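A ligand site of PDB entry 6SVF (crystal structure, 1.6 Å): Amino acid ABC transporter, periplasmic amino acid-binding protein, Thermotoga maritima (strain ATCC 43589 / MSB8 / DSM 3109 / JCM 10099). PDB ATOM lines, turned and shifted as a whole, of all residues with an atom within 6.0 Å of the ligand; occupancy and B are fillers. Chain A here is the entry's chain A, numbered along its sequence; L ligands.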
ATOM      1  N   LEU A  16      22.784   1.446  -3.847  1.00  0.00           N
ATOM      2  CA  LEU A  16      21.489   0.735  -3.914  1.00  0.00           C
ATOM      3  C   LEU A  16      20.967   0.394  -2.515  1.00  0.00           C
ATOM      4  O   LEU A  16      21.711   0.587  -1.557  1.00  0.00           O
ATOM      5  CB  LEU A  16      21.545  -0.531  -4.799  1.00  0.00           C
ATOM      6  CG  LEU A  16      22.677  -1.554  -4.521  1.00  0.00           C
ATOM      7  CD1 LEU A  16      22.348  -2.313  -3.252  1.00  0.00           C
ATOM      8  CD2 LEU A  16      22.905  -2.461  -5.676  1.00  0.00           C
ATOM      9  N   SER A  17      19.708  -0.034  -2.450  1.00  0.00           N
ATOM     10  CA  SER A  17      19.097  -0.552  -1.216  1.00  0.00           C
ATOM     11  C   SER A  17      18.761  -2.027  -1.475  1.00  0.00           C
ATOM     12  O   SER A  17      17.842  -2.360  -2.257  1.00  0.00           O
ATOM     13  CB  SER A  17      17.834   0.220  -0.888  1.00  0.00           C
ATOM     14  OG  SER A  17      17.146  -0.346   0.235  1.00  0.00           O
ATOM     15  N   ALA A  18      19.502  -2.928  -0.899  1.00  0.00           N
ATOM     16  CA  ALA A  18      19.408  -4.391  -1.224  1.00  0.00           C
ATOM     17  C   ALA A  18      18.251  -5.110  -0.429  1.00  0.00           C
ATOM     18  O   ALA A  18      18.491  -6.067   0.306  1.00  0.00           O
ATOM     19  CB  ALA A  18      20.749  -5.054  -0.955  1.00  0.00           C
ATOM     20  N   ASP A  19      17.033  -4.647  -0.655  1.00  0.00           N
ATOM     21  CA  ASP A  19      15.797  -5.155  -0.024  1.00  0.00           C
ATOM     22  C   ASP A  19      14.735  -5.253  -1.078  1.00  0.00           C
ATOM     23  O   ASP A  19      13.527  -5.141  -0.815  1.00  0.00           O
ATOM     24  CB  ASP A  19      15.316  -4.250   1.106  1.00  0.00           C
ATOM     25  CG  ASP A  19      14.860  -2.873   0.610  1.00  0.00           C
ATOM     26  OD1 ASP A  19      15.404  -2.383  -0.427  1.00  0.00           O
ATOM     27  OD2 ASP A  19      13.905  -2.287   1.265  1.00  0.00           O
ATOM     28  N   PHE A  20      15.171  -5.538  -2.320  1.00  0.00           N
ATOM     29  CA  PHE A  20      14.273  -5.350  -3.485  1.00  0.00           C
ATOM     30  C   PHE A  20      14.488  -6.423  -4.522  1.00  0.00           C
ATOM     31  O   PHE A  20      14.976  -6.169  -5.649  1.00  0.00           O
ATOM     32  CB  PHE A  20      14.513  -3.943  -4.030  1.00  0.00           C
ATOM     33  CG  PHE A  20      13.417  -3.361  -4.928  1.00  0.00           C
ATOM     34  CD1 PHE A  20      12.191  -3.007  -4.412  1.00  0.00           C
ATOM     35  CD2 PHE A  20      13.679  -3.149  -6.314  1.00  0.00           C
ATOM     36  CE1 PHE A  20      11.188  -2.449  -5.257  1.00  0.00           C
ATOM     37  CE2 PHE A  20      12.678  -2.615  -7.096  1.00  0.00           C
ATOM     38  CZ  PHE A  20      11.487  -2.220  -6.561  1.00  0.00           C
ATOM     39  N   GLU A  24      17.995  -6.165  -6.364  1.00  0.00           N
ATOM     40  CA  GLU A  24      19.146  -6.159  -5.396  1.00  0.00           C
ATOM     41  C   GLU A  24      18.604  -6.693  -4.024  1.00  0.00           C
ATOM     42  O   GLU A  24      17.620  -6.188  -3.526  1.00  0.00           O
ATOM     43  CB  GLU A  24      19.754  -4.762  -5.242  1.00  0.00           C
ATOM     44  CG  GLU A  24      18.771  -3.650  -5.022  1.00  0.00           C
ATOM     45  CD  GLU A  24      18.209  -3.066  -6.291  1.00  0.00           C
ATOM     46  OE1 GLU A  24      19.007  -3.050  -7.271  1.00  0.00           O
ATOM     47  OE2 GLU A  24      17.074  -2.561  -6.197  1.00  0.00           O
ATOM     48  N   PHE A  58      17.035   3.494   0.913  1.00  0.00           N
ATOM     49  CA  PHE A  58      16.576   3.953  -0.397  1.00  0.00           C
ATOM     50  C   PHE A  58      16.439   5.491  -0.560  1.00  0.00           C
ATOM     51  O   PHE A  58      16.888   6.093  -1.557  1.00  0.00           O
ATOM     52  CB  PHE A  58      15.303   3.247  -0.773  1.00  0.00           C
ATOM     53  CG  PHE A  58      14.801   3.662  -2.156  1.00  0.00           C
ATOM     54  CD1 PHE A  58      15.290   3.097  -3.348  1.00  0.00           C
ATOM     55  CD2 PHE A  58      13.878   4.677  -2.287  1.00  0.00           C
ATOM     56  CE1 PHE A  58      14.819   3.582  -4.608  1.00  0.00           C
ATOM     57  CE2 PHE A  58      13.355   5.127  -3.557  1.00  0.00           C
ATOM     58  CZ  PHE A  58      13.880   4.599  -4.706  1.00  0.00           C
ATOM     59  N   LEU A  61      19.640   7.545  -1.361  1.00  0.00           N
ATOM     60  CA  LEU A  61      20.386   7.358  -2.618  1.00  0.00           C
ATOM     61  C   LEU A  61      20.599   8.638  -3.373  1.00  0.00           C
ATOM     62  O   LEU A  61      21.726   8.977  -3.733  1.00  0.00           O
ATOM     63  CB  LEU A  61      19.666   6.338  -3.464  1.00  0.00           C
ATOM     64  CG  LEU A  61      19.730   4.904  -2.933  1.00  0.00           C
ATOM     65  CD1 LEU A  61      18.687   4.076  -3.640  1.00  0.00           C
ATOM     66  CD2 LEU A  61      21.073   4.223  -3.147  1.00  0.00           C
ATOM     67  N   SER A  75      19.157   0.802  -8.594  1.00  0.00           N
ATOM     68  CA  SER A  75      18.455   0.386  -7.393  1.00  0.00           C
ATOM     69  C   SER A  75      16.947   0.310  -7.626  1.00  0.00           C
ATOM     70  O   SER A  75      16.152   0.616  -6.771  1.00  0.00           O
ATOM     71  CB  SER A  75      18.811   1.277  -6.222  1.00  0.00           C
ATOM     72  OG  SER A  75      18.341   0.718  -5.007  1.00  0.00           O
ATOM     73  N   GLY A  76      16.563  -0.183  -8.787  1.00  0.00           N
ATOM     74  CA  GLY A  76      15.156  -0.292  -9.075  1.00  0.00           C
ATOM     75  C   GLY A  76      14.470   1.018  -9.127  1.00  0.00           C
ATOM     76  O   GLY A  76      13.269   1.102  -8.769  1.00  0.00           O
ATOM     77  N   MET A  77      15.175   2.052  -9.572  1.00  0.00           N
ATOM     78  CA  MET A  77      14.668   3.431  -9.449  1.00  0.00           C
ATOM     79  C   MET A  77      13.814   3.849 -10.631  1.00  0.00           C
ATOM     80  O   MET A  77      14.341   3.905 -11.761  1.00  0.00           O
ATOM     81  CB  MET A  77      15.814   4.407  -9.206  1.00  0.00           C
ATOM     82  CG  MET A  77      15.276   5.799  -8.865  1.00  0.00           C
ATOM     83  SD  MET A  77      16.563   6.935  -8.333  1.00  0.00           S
ATOM     84  CE  MET A  77      16.502   6.632  -6.571  1.00  0.00           C
ATOM     85  N   THR A  78      12.610   4.239 -10.311  1.00  0.00           N
ATOM     86  CA  THR A  78      11.678   4.791 -11.327  1.00  0.00           C
ATOM     87  C   THR A  78      12.139   6.181 -11.826  1.00  0.00           C
ATOM     88  O   THR A  78      12.463   7.067 -11.036  1.00  0.00           O
ATOM     89  CB  THR A  78      10.278   4.892 -10.734  1.00  0.00           C
ATOM     90  OG1 THR A  78       9.836   3.577 -10.484  1.00  0.00           O
ATOM     91  CG2 THR A  78       9.304   5.508 -11.735  1.00  0.00           C
ATOM     92  N   ILE A  79      12.098   6.299 -13.142  1.00  0.00           N
ATOM     93  CA  ILE A  79      12.254   7.620 -13.787  1.00  0.00           C
ATOM     94  C   ILE A  79      11.033   8.435 -13.540  1.00  0.00           C
ATOM     95  O   ILE A  79       9.935   8.093 -14.012  1.00  0.00           O
ATOM     96  CB  ILE A  79      12.574   7.470 -15.301  1.00  0.00           C
ATOM     97  CG1 ILE A  79      13.779   6.523 -15.540  1.00  0.00           C
ATOM     98  CG2 ILE A  79      12.772   8.846 -15.945  1.00  0.00           C
ATOM     99  CD1 ILE A  79      13.854   5.961 -16.991  1.00  0.00           C
ATOM    100  N   ARG A  83      12.208  13.574  -9.985  1.00  0.00           N
ATOM    101  CA  ARG A  83      13.604  13.238  -9.792  1.00  0.00           C
ATOM    102  C   ARG A  83      14.469  13.803 -10.917  1.00  0.00           C
ATOM    103  O   ARG A  83      15.642  14.155 -10.704  1.00  0.00           O
ATOM    104  CB  ARG A  83      13.804  11.732  -9.662  1.00  0.00           C
ATOM    105  CG  ARG A  83      13.245  11.168  -8.369  1.00  0.00           C
ATOM    106  CD  ARG A  83      13.095   9.653  -8.462  1.00  0.00           C
ATOM    107  NE  ARG A  83      12.535   9.078  -7.250  1.00  0.00           N
ATOM    108  CZ  ARG A  83      12.095   7.816  -7.115  1.00  0.00           C
ATOM    109  NH1 ARG A  83      12.073   6.974  -8.118  1.00  0.00           N
ATOM    110  NH2 ARG A  83      11.637   7.401  -5.943  1.00  0.00           N
ATOM    111  N   GLN A  98       2.813   0.069  -9.445  1.00  0.00           N
ATOM    112  CA  GLN A  98       2.494  -0.277  -8.085  1.00  0.00           C
ATOM    113  C   GLN A  98       1.374  -1.285  -8.043  1.00  0.00           C
ATOM    114  O   GLN A  98       0.454  -1.230  -8.865  1.00  0.00           O
ATOM    115  CB  GLN A  98       2.090   0.944  -7.242  1.00  0.00           C
ATOM    116  CG  GLN A  98       3.089   2.092  -7.199  1.00  0.00           C
ATOM    117  CD  GLN A  98       4.432   1.614  -6.715  1.00  0.00           C
ATOM    118  OE1 GLN A  98       4.522   1.112  -5.576  1.00  0.00           O
ATOM    119  NE2 GLN A  98       5.483   1.692  -7.575  1.00  0.00           N
ATOM    120  N   GLN A 124       7.751   1.747   1.549  1.00  0.00           N
ATOM    121  CA  GLN A 124       9.192   2.116   1.809  1.00  0.00           C
ATOM    122  C   GLN A 124       9.253   3.617   1.639  1.00  0.00           C
ATOM    123  O   GLN A 124       8.853   4.190   0.629  1.00  0.00           O
ATOM    124  CB  GLN A 124      10.051   1.430   0.802  1.00  0.00           C
ATOM    125  CG  GLN A 124      11.500   1.932   0.822  1.00  0.00           C
ATOM    126  CD  GLN A 124      12.411   1.013   0.072  1.00  0.00           C
ATOM    127  OE1 GLN A 124      12.386   1.032  -1.132  1.00  0.00           O
ATOM    128  NE2 GLN A 124      13.290   0.281   0.819  1.00  0.00           N
ATOM    129  N   GLY A 126      10.083   7.217   0.691  1.00  0.00           N
ATOM    130  CA  GLY A 126      10.719   7.798  -0.451  1.00  0.00           C
ATOM    131  C   GLY A 126      10.404   7.174  -1.774  1.00  0.00           C
ATOM    132  O   GLY A 126      10.893   7.656  -2.798  1.00  0.00           O
ATOM    133  N   THR A 127       9.685   6.073  -1.769  1.00  0.00           N
ATOM    134  CA  THR A 127       9.349   5.409  -3.061  1.00  0.00           C
ATOM    135  C   THR A 127       8.138   6.047  -3.793  1.00  0.00           C
ATOM    136  O   THR A 127       7.368   6.797  -3.181  1.00  0.00           O
ATOM    137  CB  THR A 127       9.052   3.952  -2.850  1.00  0.00           C
ATOM    138  OG1 THR A 127       7.989   3.796  -1.899  1.00  0.00           O
ATOM    139  CG2 THR A 127      10.329   3.225  -2.356  1.00  0.00           C
ATOM    140  N   THR A 128       7.966   5.687  -5.057  1.00  0.00           N
ATOM    141  CA  THR A 128       6.789   6.053  -5.799  1.00  0.00           C
ATOM    142  C   THR A 128       5.533   5.528  -5.130  1.00  0.00           C
ATOM    143  O   THR A 128       4.471   6.201  -5.179  1.00  0.00           O
ATOM    144  CB  THR A 128       6.922   5.629  -7.249  1.00  0.00           C
ATOM    145  OG1 THR A 128       7.297   4.230  -7.301  1.00  0.00           O
ATOM    146  CG2 THR A 128       7.997   6.381  -7.976  1.00  0.00           C
ATOM    147  N   GLY A 129       5.592   4.381  -4.479  1.00  0.00           N
ATOM    148  CA  GLY A 129       4.436   3.859  -3.693  1.00  0.00           C
ATOM    149  C   GLY A 129       4.129   4.813  -2.534  1.00  0.00           C
ATOM    150  O   GLY A 129       2.972   5.156  -2.317  1.00  0.00           O
ATOM    151  N   PHE A 147      11.817  -3.071   2.894  1.00  0.00           N
ATOM    152  CA  PHE A 147      10.582  -3.800   2.534  1.00  0.00           C
ATOM    153  C   PHE A 147      10.439  -5.023   3.426  1.00  0.00           C
ATOM    154  O   PHE A 147       9.338  -5.497   3.698  1.00  0.00           O
ATOM    155  CB  PHE A 147      10.582  -4.151   1.035  1.00  0.00           C
ATOM    156  CG  PHE A 147      10.087  -3.077   0.175  1.00  0.00           C
ATOM    157  CD1 PHE A 147       8.796  -2.630   0.302  1.00  0.00           C
ATOM    158  CD2 PHE A 147      10.896  -2.479  -0.791  1.00  0.00           C
ATOM    159  CE1 PHE A 147       8.315  -1.619  -0.473  1.00  0.00           C
ATOM    160  CE2 PHE A 147      10.438  -1.510  -1.585  1.00  0.00           C
ATOM    161  CZ  PHE A 147       9.137  -1.046  -1.443  1.00  0.00           C
ATOM    162  N   ASP A 165       6.152  -1.932  -5.959  1.00  0.00           N
ATOM    163  CA  ASP A 165       6.321  -2.292  -7.381  1.00  0.00           C
ATOM    164  C   ASP A 165       6.004  -3.793  -7.612  1.00  0.00           C
ATOM    165  O   ASP A 165       6.399  -4.681  -6.830  1.00  0.00           O
ATOM    166  CB  ASP A 165       7.758  -2.046  -7.877  1.00  0.00           C
ATOM    167  CG  ASP A 165       8.287  -0.613  -7.716  1.00  0.00           C
ATOM    168  OD1 ASP A 165       7.966   0.067  -6.763  1.00  0.00           O
ATOM    169  OD2 ASP A 165       9.048  -0.203  -8.634  1.00  0.00           O
ATOM    170  N   GLU A 189       5.445   2.649 -14.699  1.00  0.00           N
ATOM    171  CA  GLU A 189       6.745   3.099 -14.355  1.00  0.00           C
ATOM    172  C   GLU A 189       7.840   2.371 -15.167  1.00  0.00           C
ATOM    173  O   GLU A 189       7.649   1.228 -15.580  1.00  0.00           O
ATOM    174  CB  GLU A 189       6.987   2.945 -12.847  1.00  0.00           C
ATOM    175  CG  GLU A 189       5.956   3.627 -12.043  1.00  0.00           C
ATOM    176  CD  GLU A 189       6.047   3.518 -10.510  1.00  0.00           C
ATOM    177  OE1 GLU A 189       7.179   3.503  -9.976  1.00  0.00           O
ATOM    178  OE2 GLU A 189       4.970   3.440  -9.894  1.00  0.00           O
ATOM    179  N   TYR A 191      12.269   1.816 -14.964  1.00  0.00           N
ATOM    180  CA  TYR A 191      13.489   1.976 -14.158  1.00  0.00           C
ATOM    181  C   TYR A 191      14.556   2.590 -15.011  1.00  0.00           C
ATOM    182  O   TYR A 191      14.733   2.206 -16.211  1.00  0.00           O
ATOM    183  CB  TYR A 191      14.048   0.684 -13.549  1.00  0.00           C
ATOM    184  CG  TYR A 191      13.068  -0.026 -12.567  1.00  0.00           C
ATOM    185  CD1 TYR A 191      11.935   0.611 -12.071  1.00  0.00           C
ATOM    186  CD2 TYR A 191      13.269  -1.309 -12.203  1.00  0.00           C
ATOM    187  CE1 TYR A 191      11.035  -0.080 -11.236  1.00  0.00           C
ATOM    188  CE2 TYR A 191      12.449  -1.972 -11.325  1.00  0.00           C
ATOM    189  CZ  TYR A 191      11.309  -1.370 -10.844  1.00  0.00           C
ATOM    190  OH  TYR A 191      10.427  -2.004  -9.945  1.00  0.00           O
HETATM  191  N1  LIG L   1      10.650   1.960  -8.216  1.00  0.00           N
HETATM  192  C1  LIG L   1      10.329   2.514  -6.840  1.00  0.00           C
HETATM  193  C2  LIG L   1      10.893   3.938  -6.804  1.00  0.00           C
HETATM  194  O1  LIG L   1      11.770   4.293  -7.653  1.00  0.00           O
HETATM  195  C3  LIG L   1      10.850   1.643  -5.688  1.00  0.00           C
HETATM  196  C4  LIG L   1      12.305   1.312  -5.780  1.00  0.00           C
HETATM  197  C5  LIG L   1      12.834   0.806  -4.445  1.00  0.00           C
HETATM  198  N2  LIG L   1      14.155   0.179  -4.667  1.00  0.00           N
HETATM  199  C6  LIG L   1      14.824  -0.435  -3.705  1.00  0.00           C
HETATM  200  N3  LIG L   1      14.312  -0.452  -2.461  1.00  0.00           N
HETATM  201  N4  LIG L   1      15.986  -1.022  -4.002  1.00  0.00           N
HETATM  202  O2  LIG L   1      10.495   4.648  -5.904  1.00  0.00           O
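Phe 20 touches the ligand.
Phe 58 touches the ligand (CD1 to N2, 3.4 Å).
Met 77 touches the ligand.
CA of Thr 127 touches O2 of the ligand (3.2 Å).
Tyr 191 touches the ligand (CE1 to N1, 3.7 Å).
Of the 24 residues printed, 15 come within 4 Å of the ligand.
The nearest printed residue that does not touch the ligand is Phe 147 (4.1 Å).
OG1 of Thr 128 lies within hydrogen-bond range of OE1 of Glu 189 (2.8 Å).
The side-chain carboxylate of Asp 19 sits at hydrogen-bond distance from the backbone NH of Phe 147, at 2.8 Å.
The side-chain hydroxyl (OG) of Ser 75 lies within hydrogen-bond range of the backbone NH (N) of Ser 17 (3.0 Å).
O of Glu 24 is in hydrogen-bond range of N of Asp 19 (3.3 Å).
The backbone carbonyl oxygen of Gln 124 is in hydrogen-bond range of the side-chain hydroxyl of Thr 127 (2.7 Å).
The guanidinium group (NH2) of Arg 83 is in hydrogen-bond range of the backbone carbonyl oxygen (O) of Gly 126.
OG1 of Thr 78 lies within hydrogen-bond range of OE1 of Glu 189 (2.7 Å).
OG of Ser 17 is in hydrogen-bond range of OD1 of Asp 19 (2.8 Å).
N3 of the ligand lies within salt-bridge range of OD1 of Asp 19, 3.0 Å away.
OG of Ser 75 sits at hydrogen-bond distance from N4 of the ligand (3.1 Å).
The side-chain carboxylate of Glu 24 lies within salt-bridge range of a nitrogen (N4) of the ligand (2.9 Å).
The backbone carbonyl oxygen of Ser 75 is in hydrogen-bond range of a nitrogen (N2) of the ligand (2.9 Å).
OD2 of Asp 165 lies within salt-bridge range of N1 of the ligand.
OG1 of Thr 78 is in hydrogen-bond range of N1 of the ligand, 2.9 Å away.
The guanidinium group (NH1) of Arg 83 lies within salt-bridge range of an oxygen (O1) of the ligand.
The backbone carbonyl oxygen (O) of Ser 17 sits at hydrogen-bond distance from a nitrogen (N4) of the ligand (2.9 Å).
A nitrogen (N3) of the ligand is in hydrogen-bond range of the side-chain amide oxygen (OE1) of Gln 124.
An oxygen (O1) of the ligand is in hydrogen-bond range of the backbone NH (N) of Thr 78, at 2.8 Å.
The backbone carbonyl oxygen (O) of Gly 76 lies within hydrogen-bond range of a nitrogen (N1) of the ligand (2.8 Å).
The backbone NH (N) of Thr 128 lies within hydrogen-bond range of an oxygen (O2) of the ligand.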
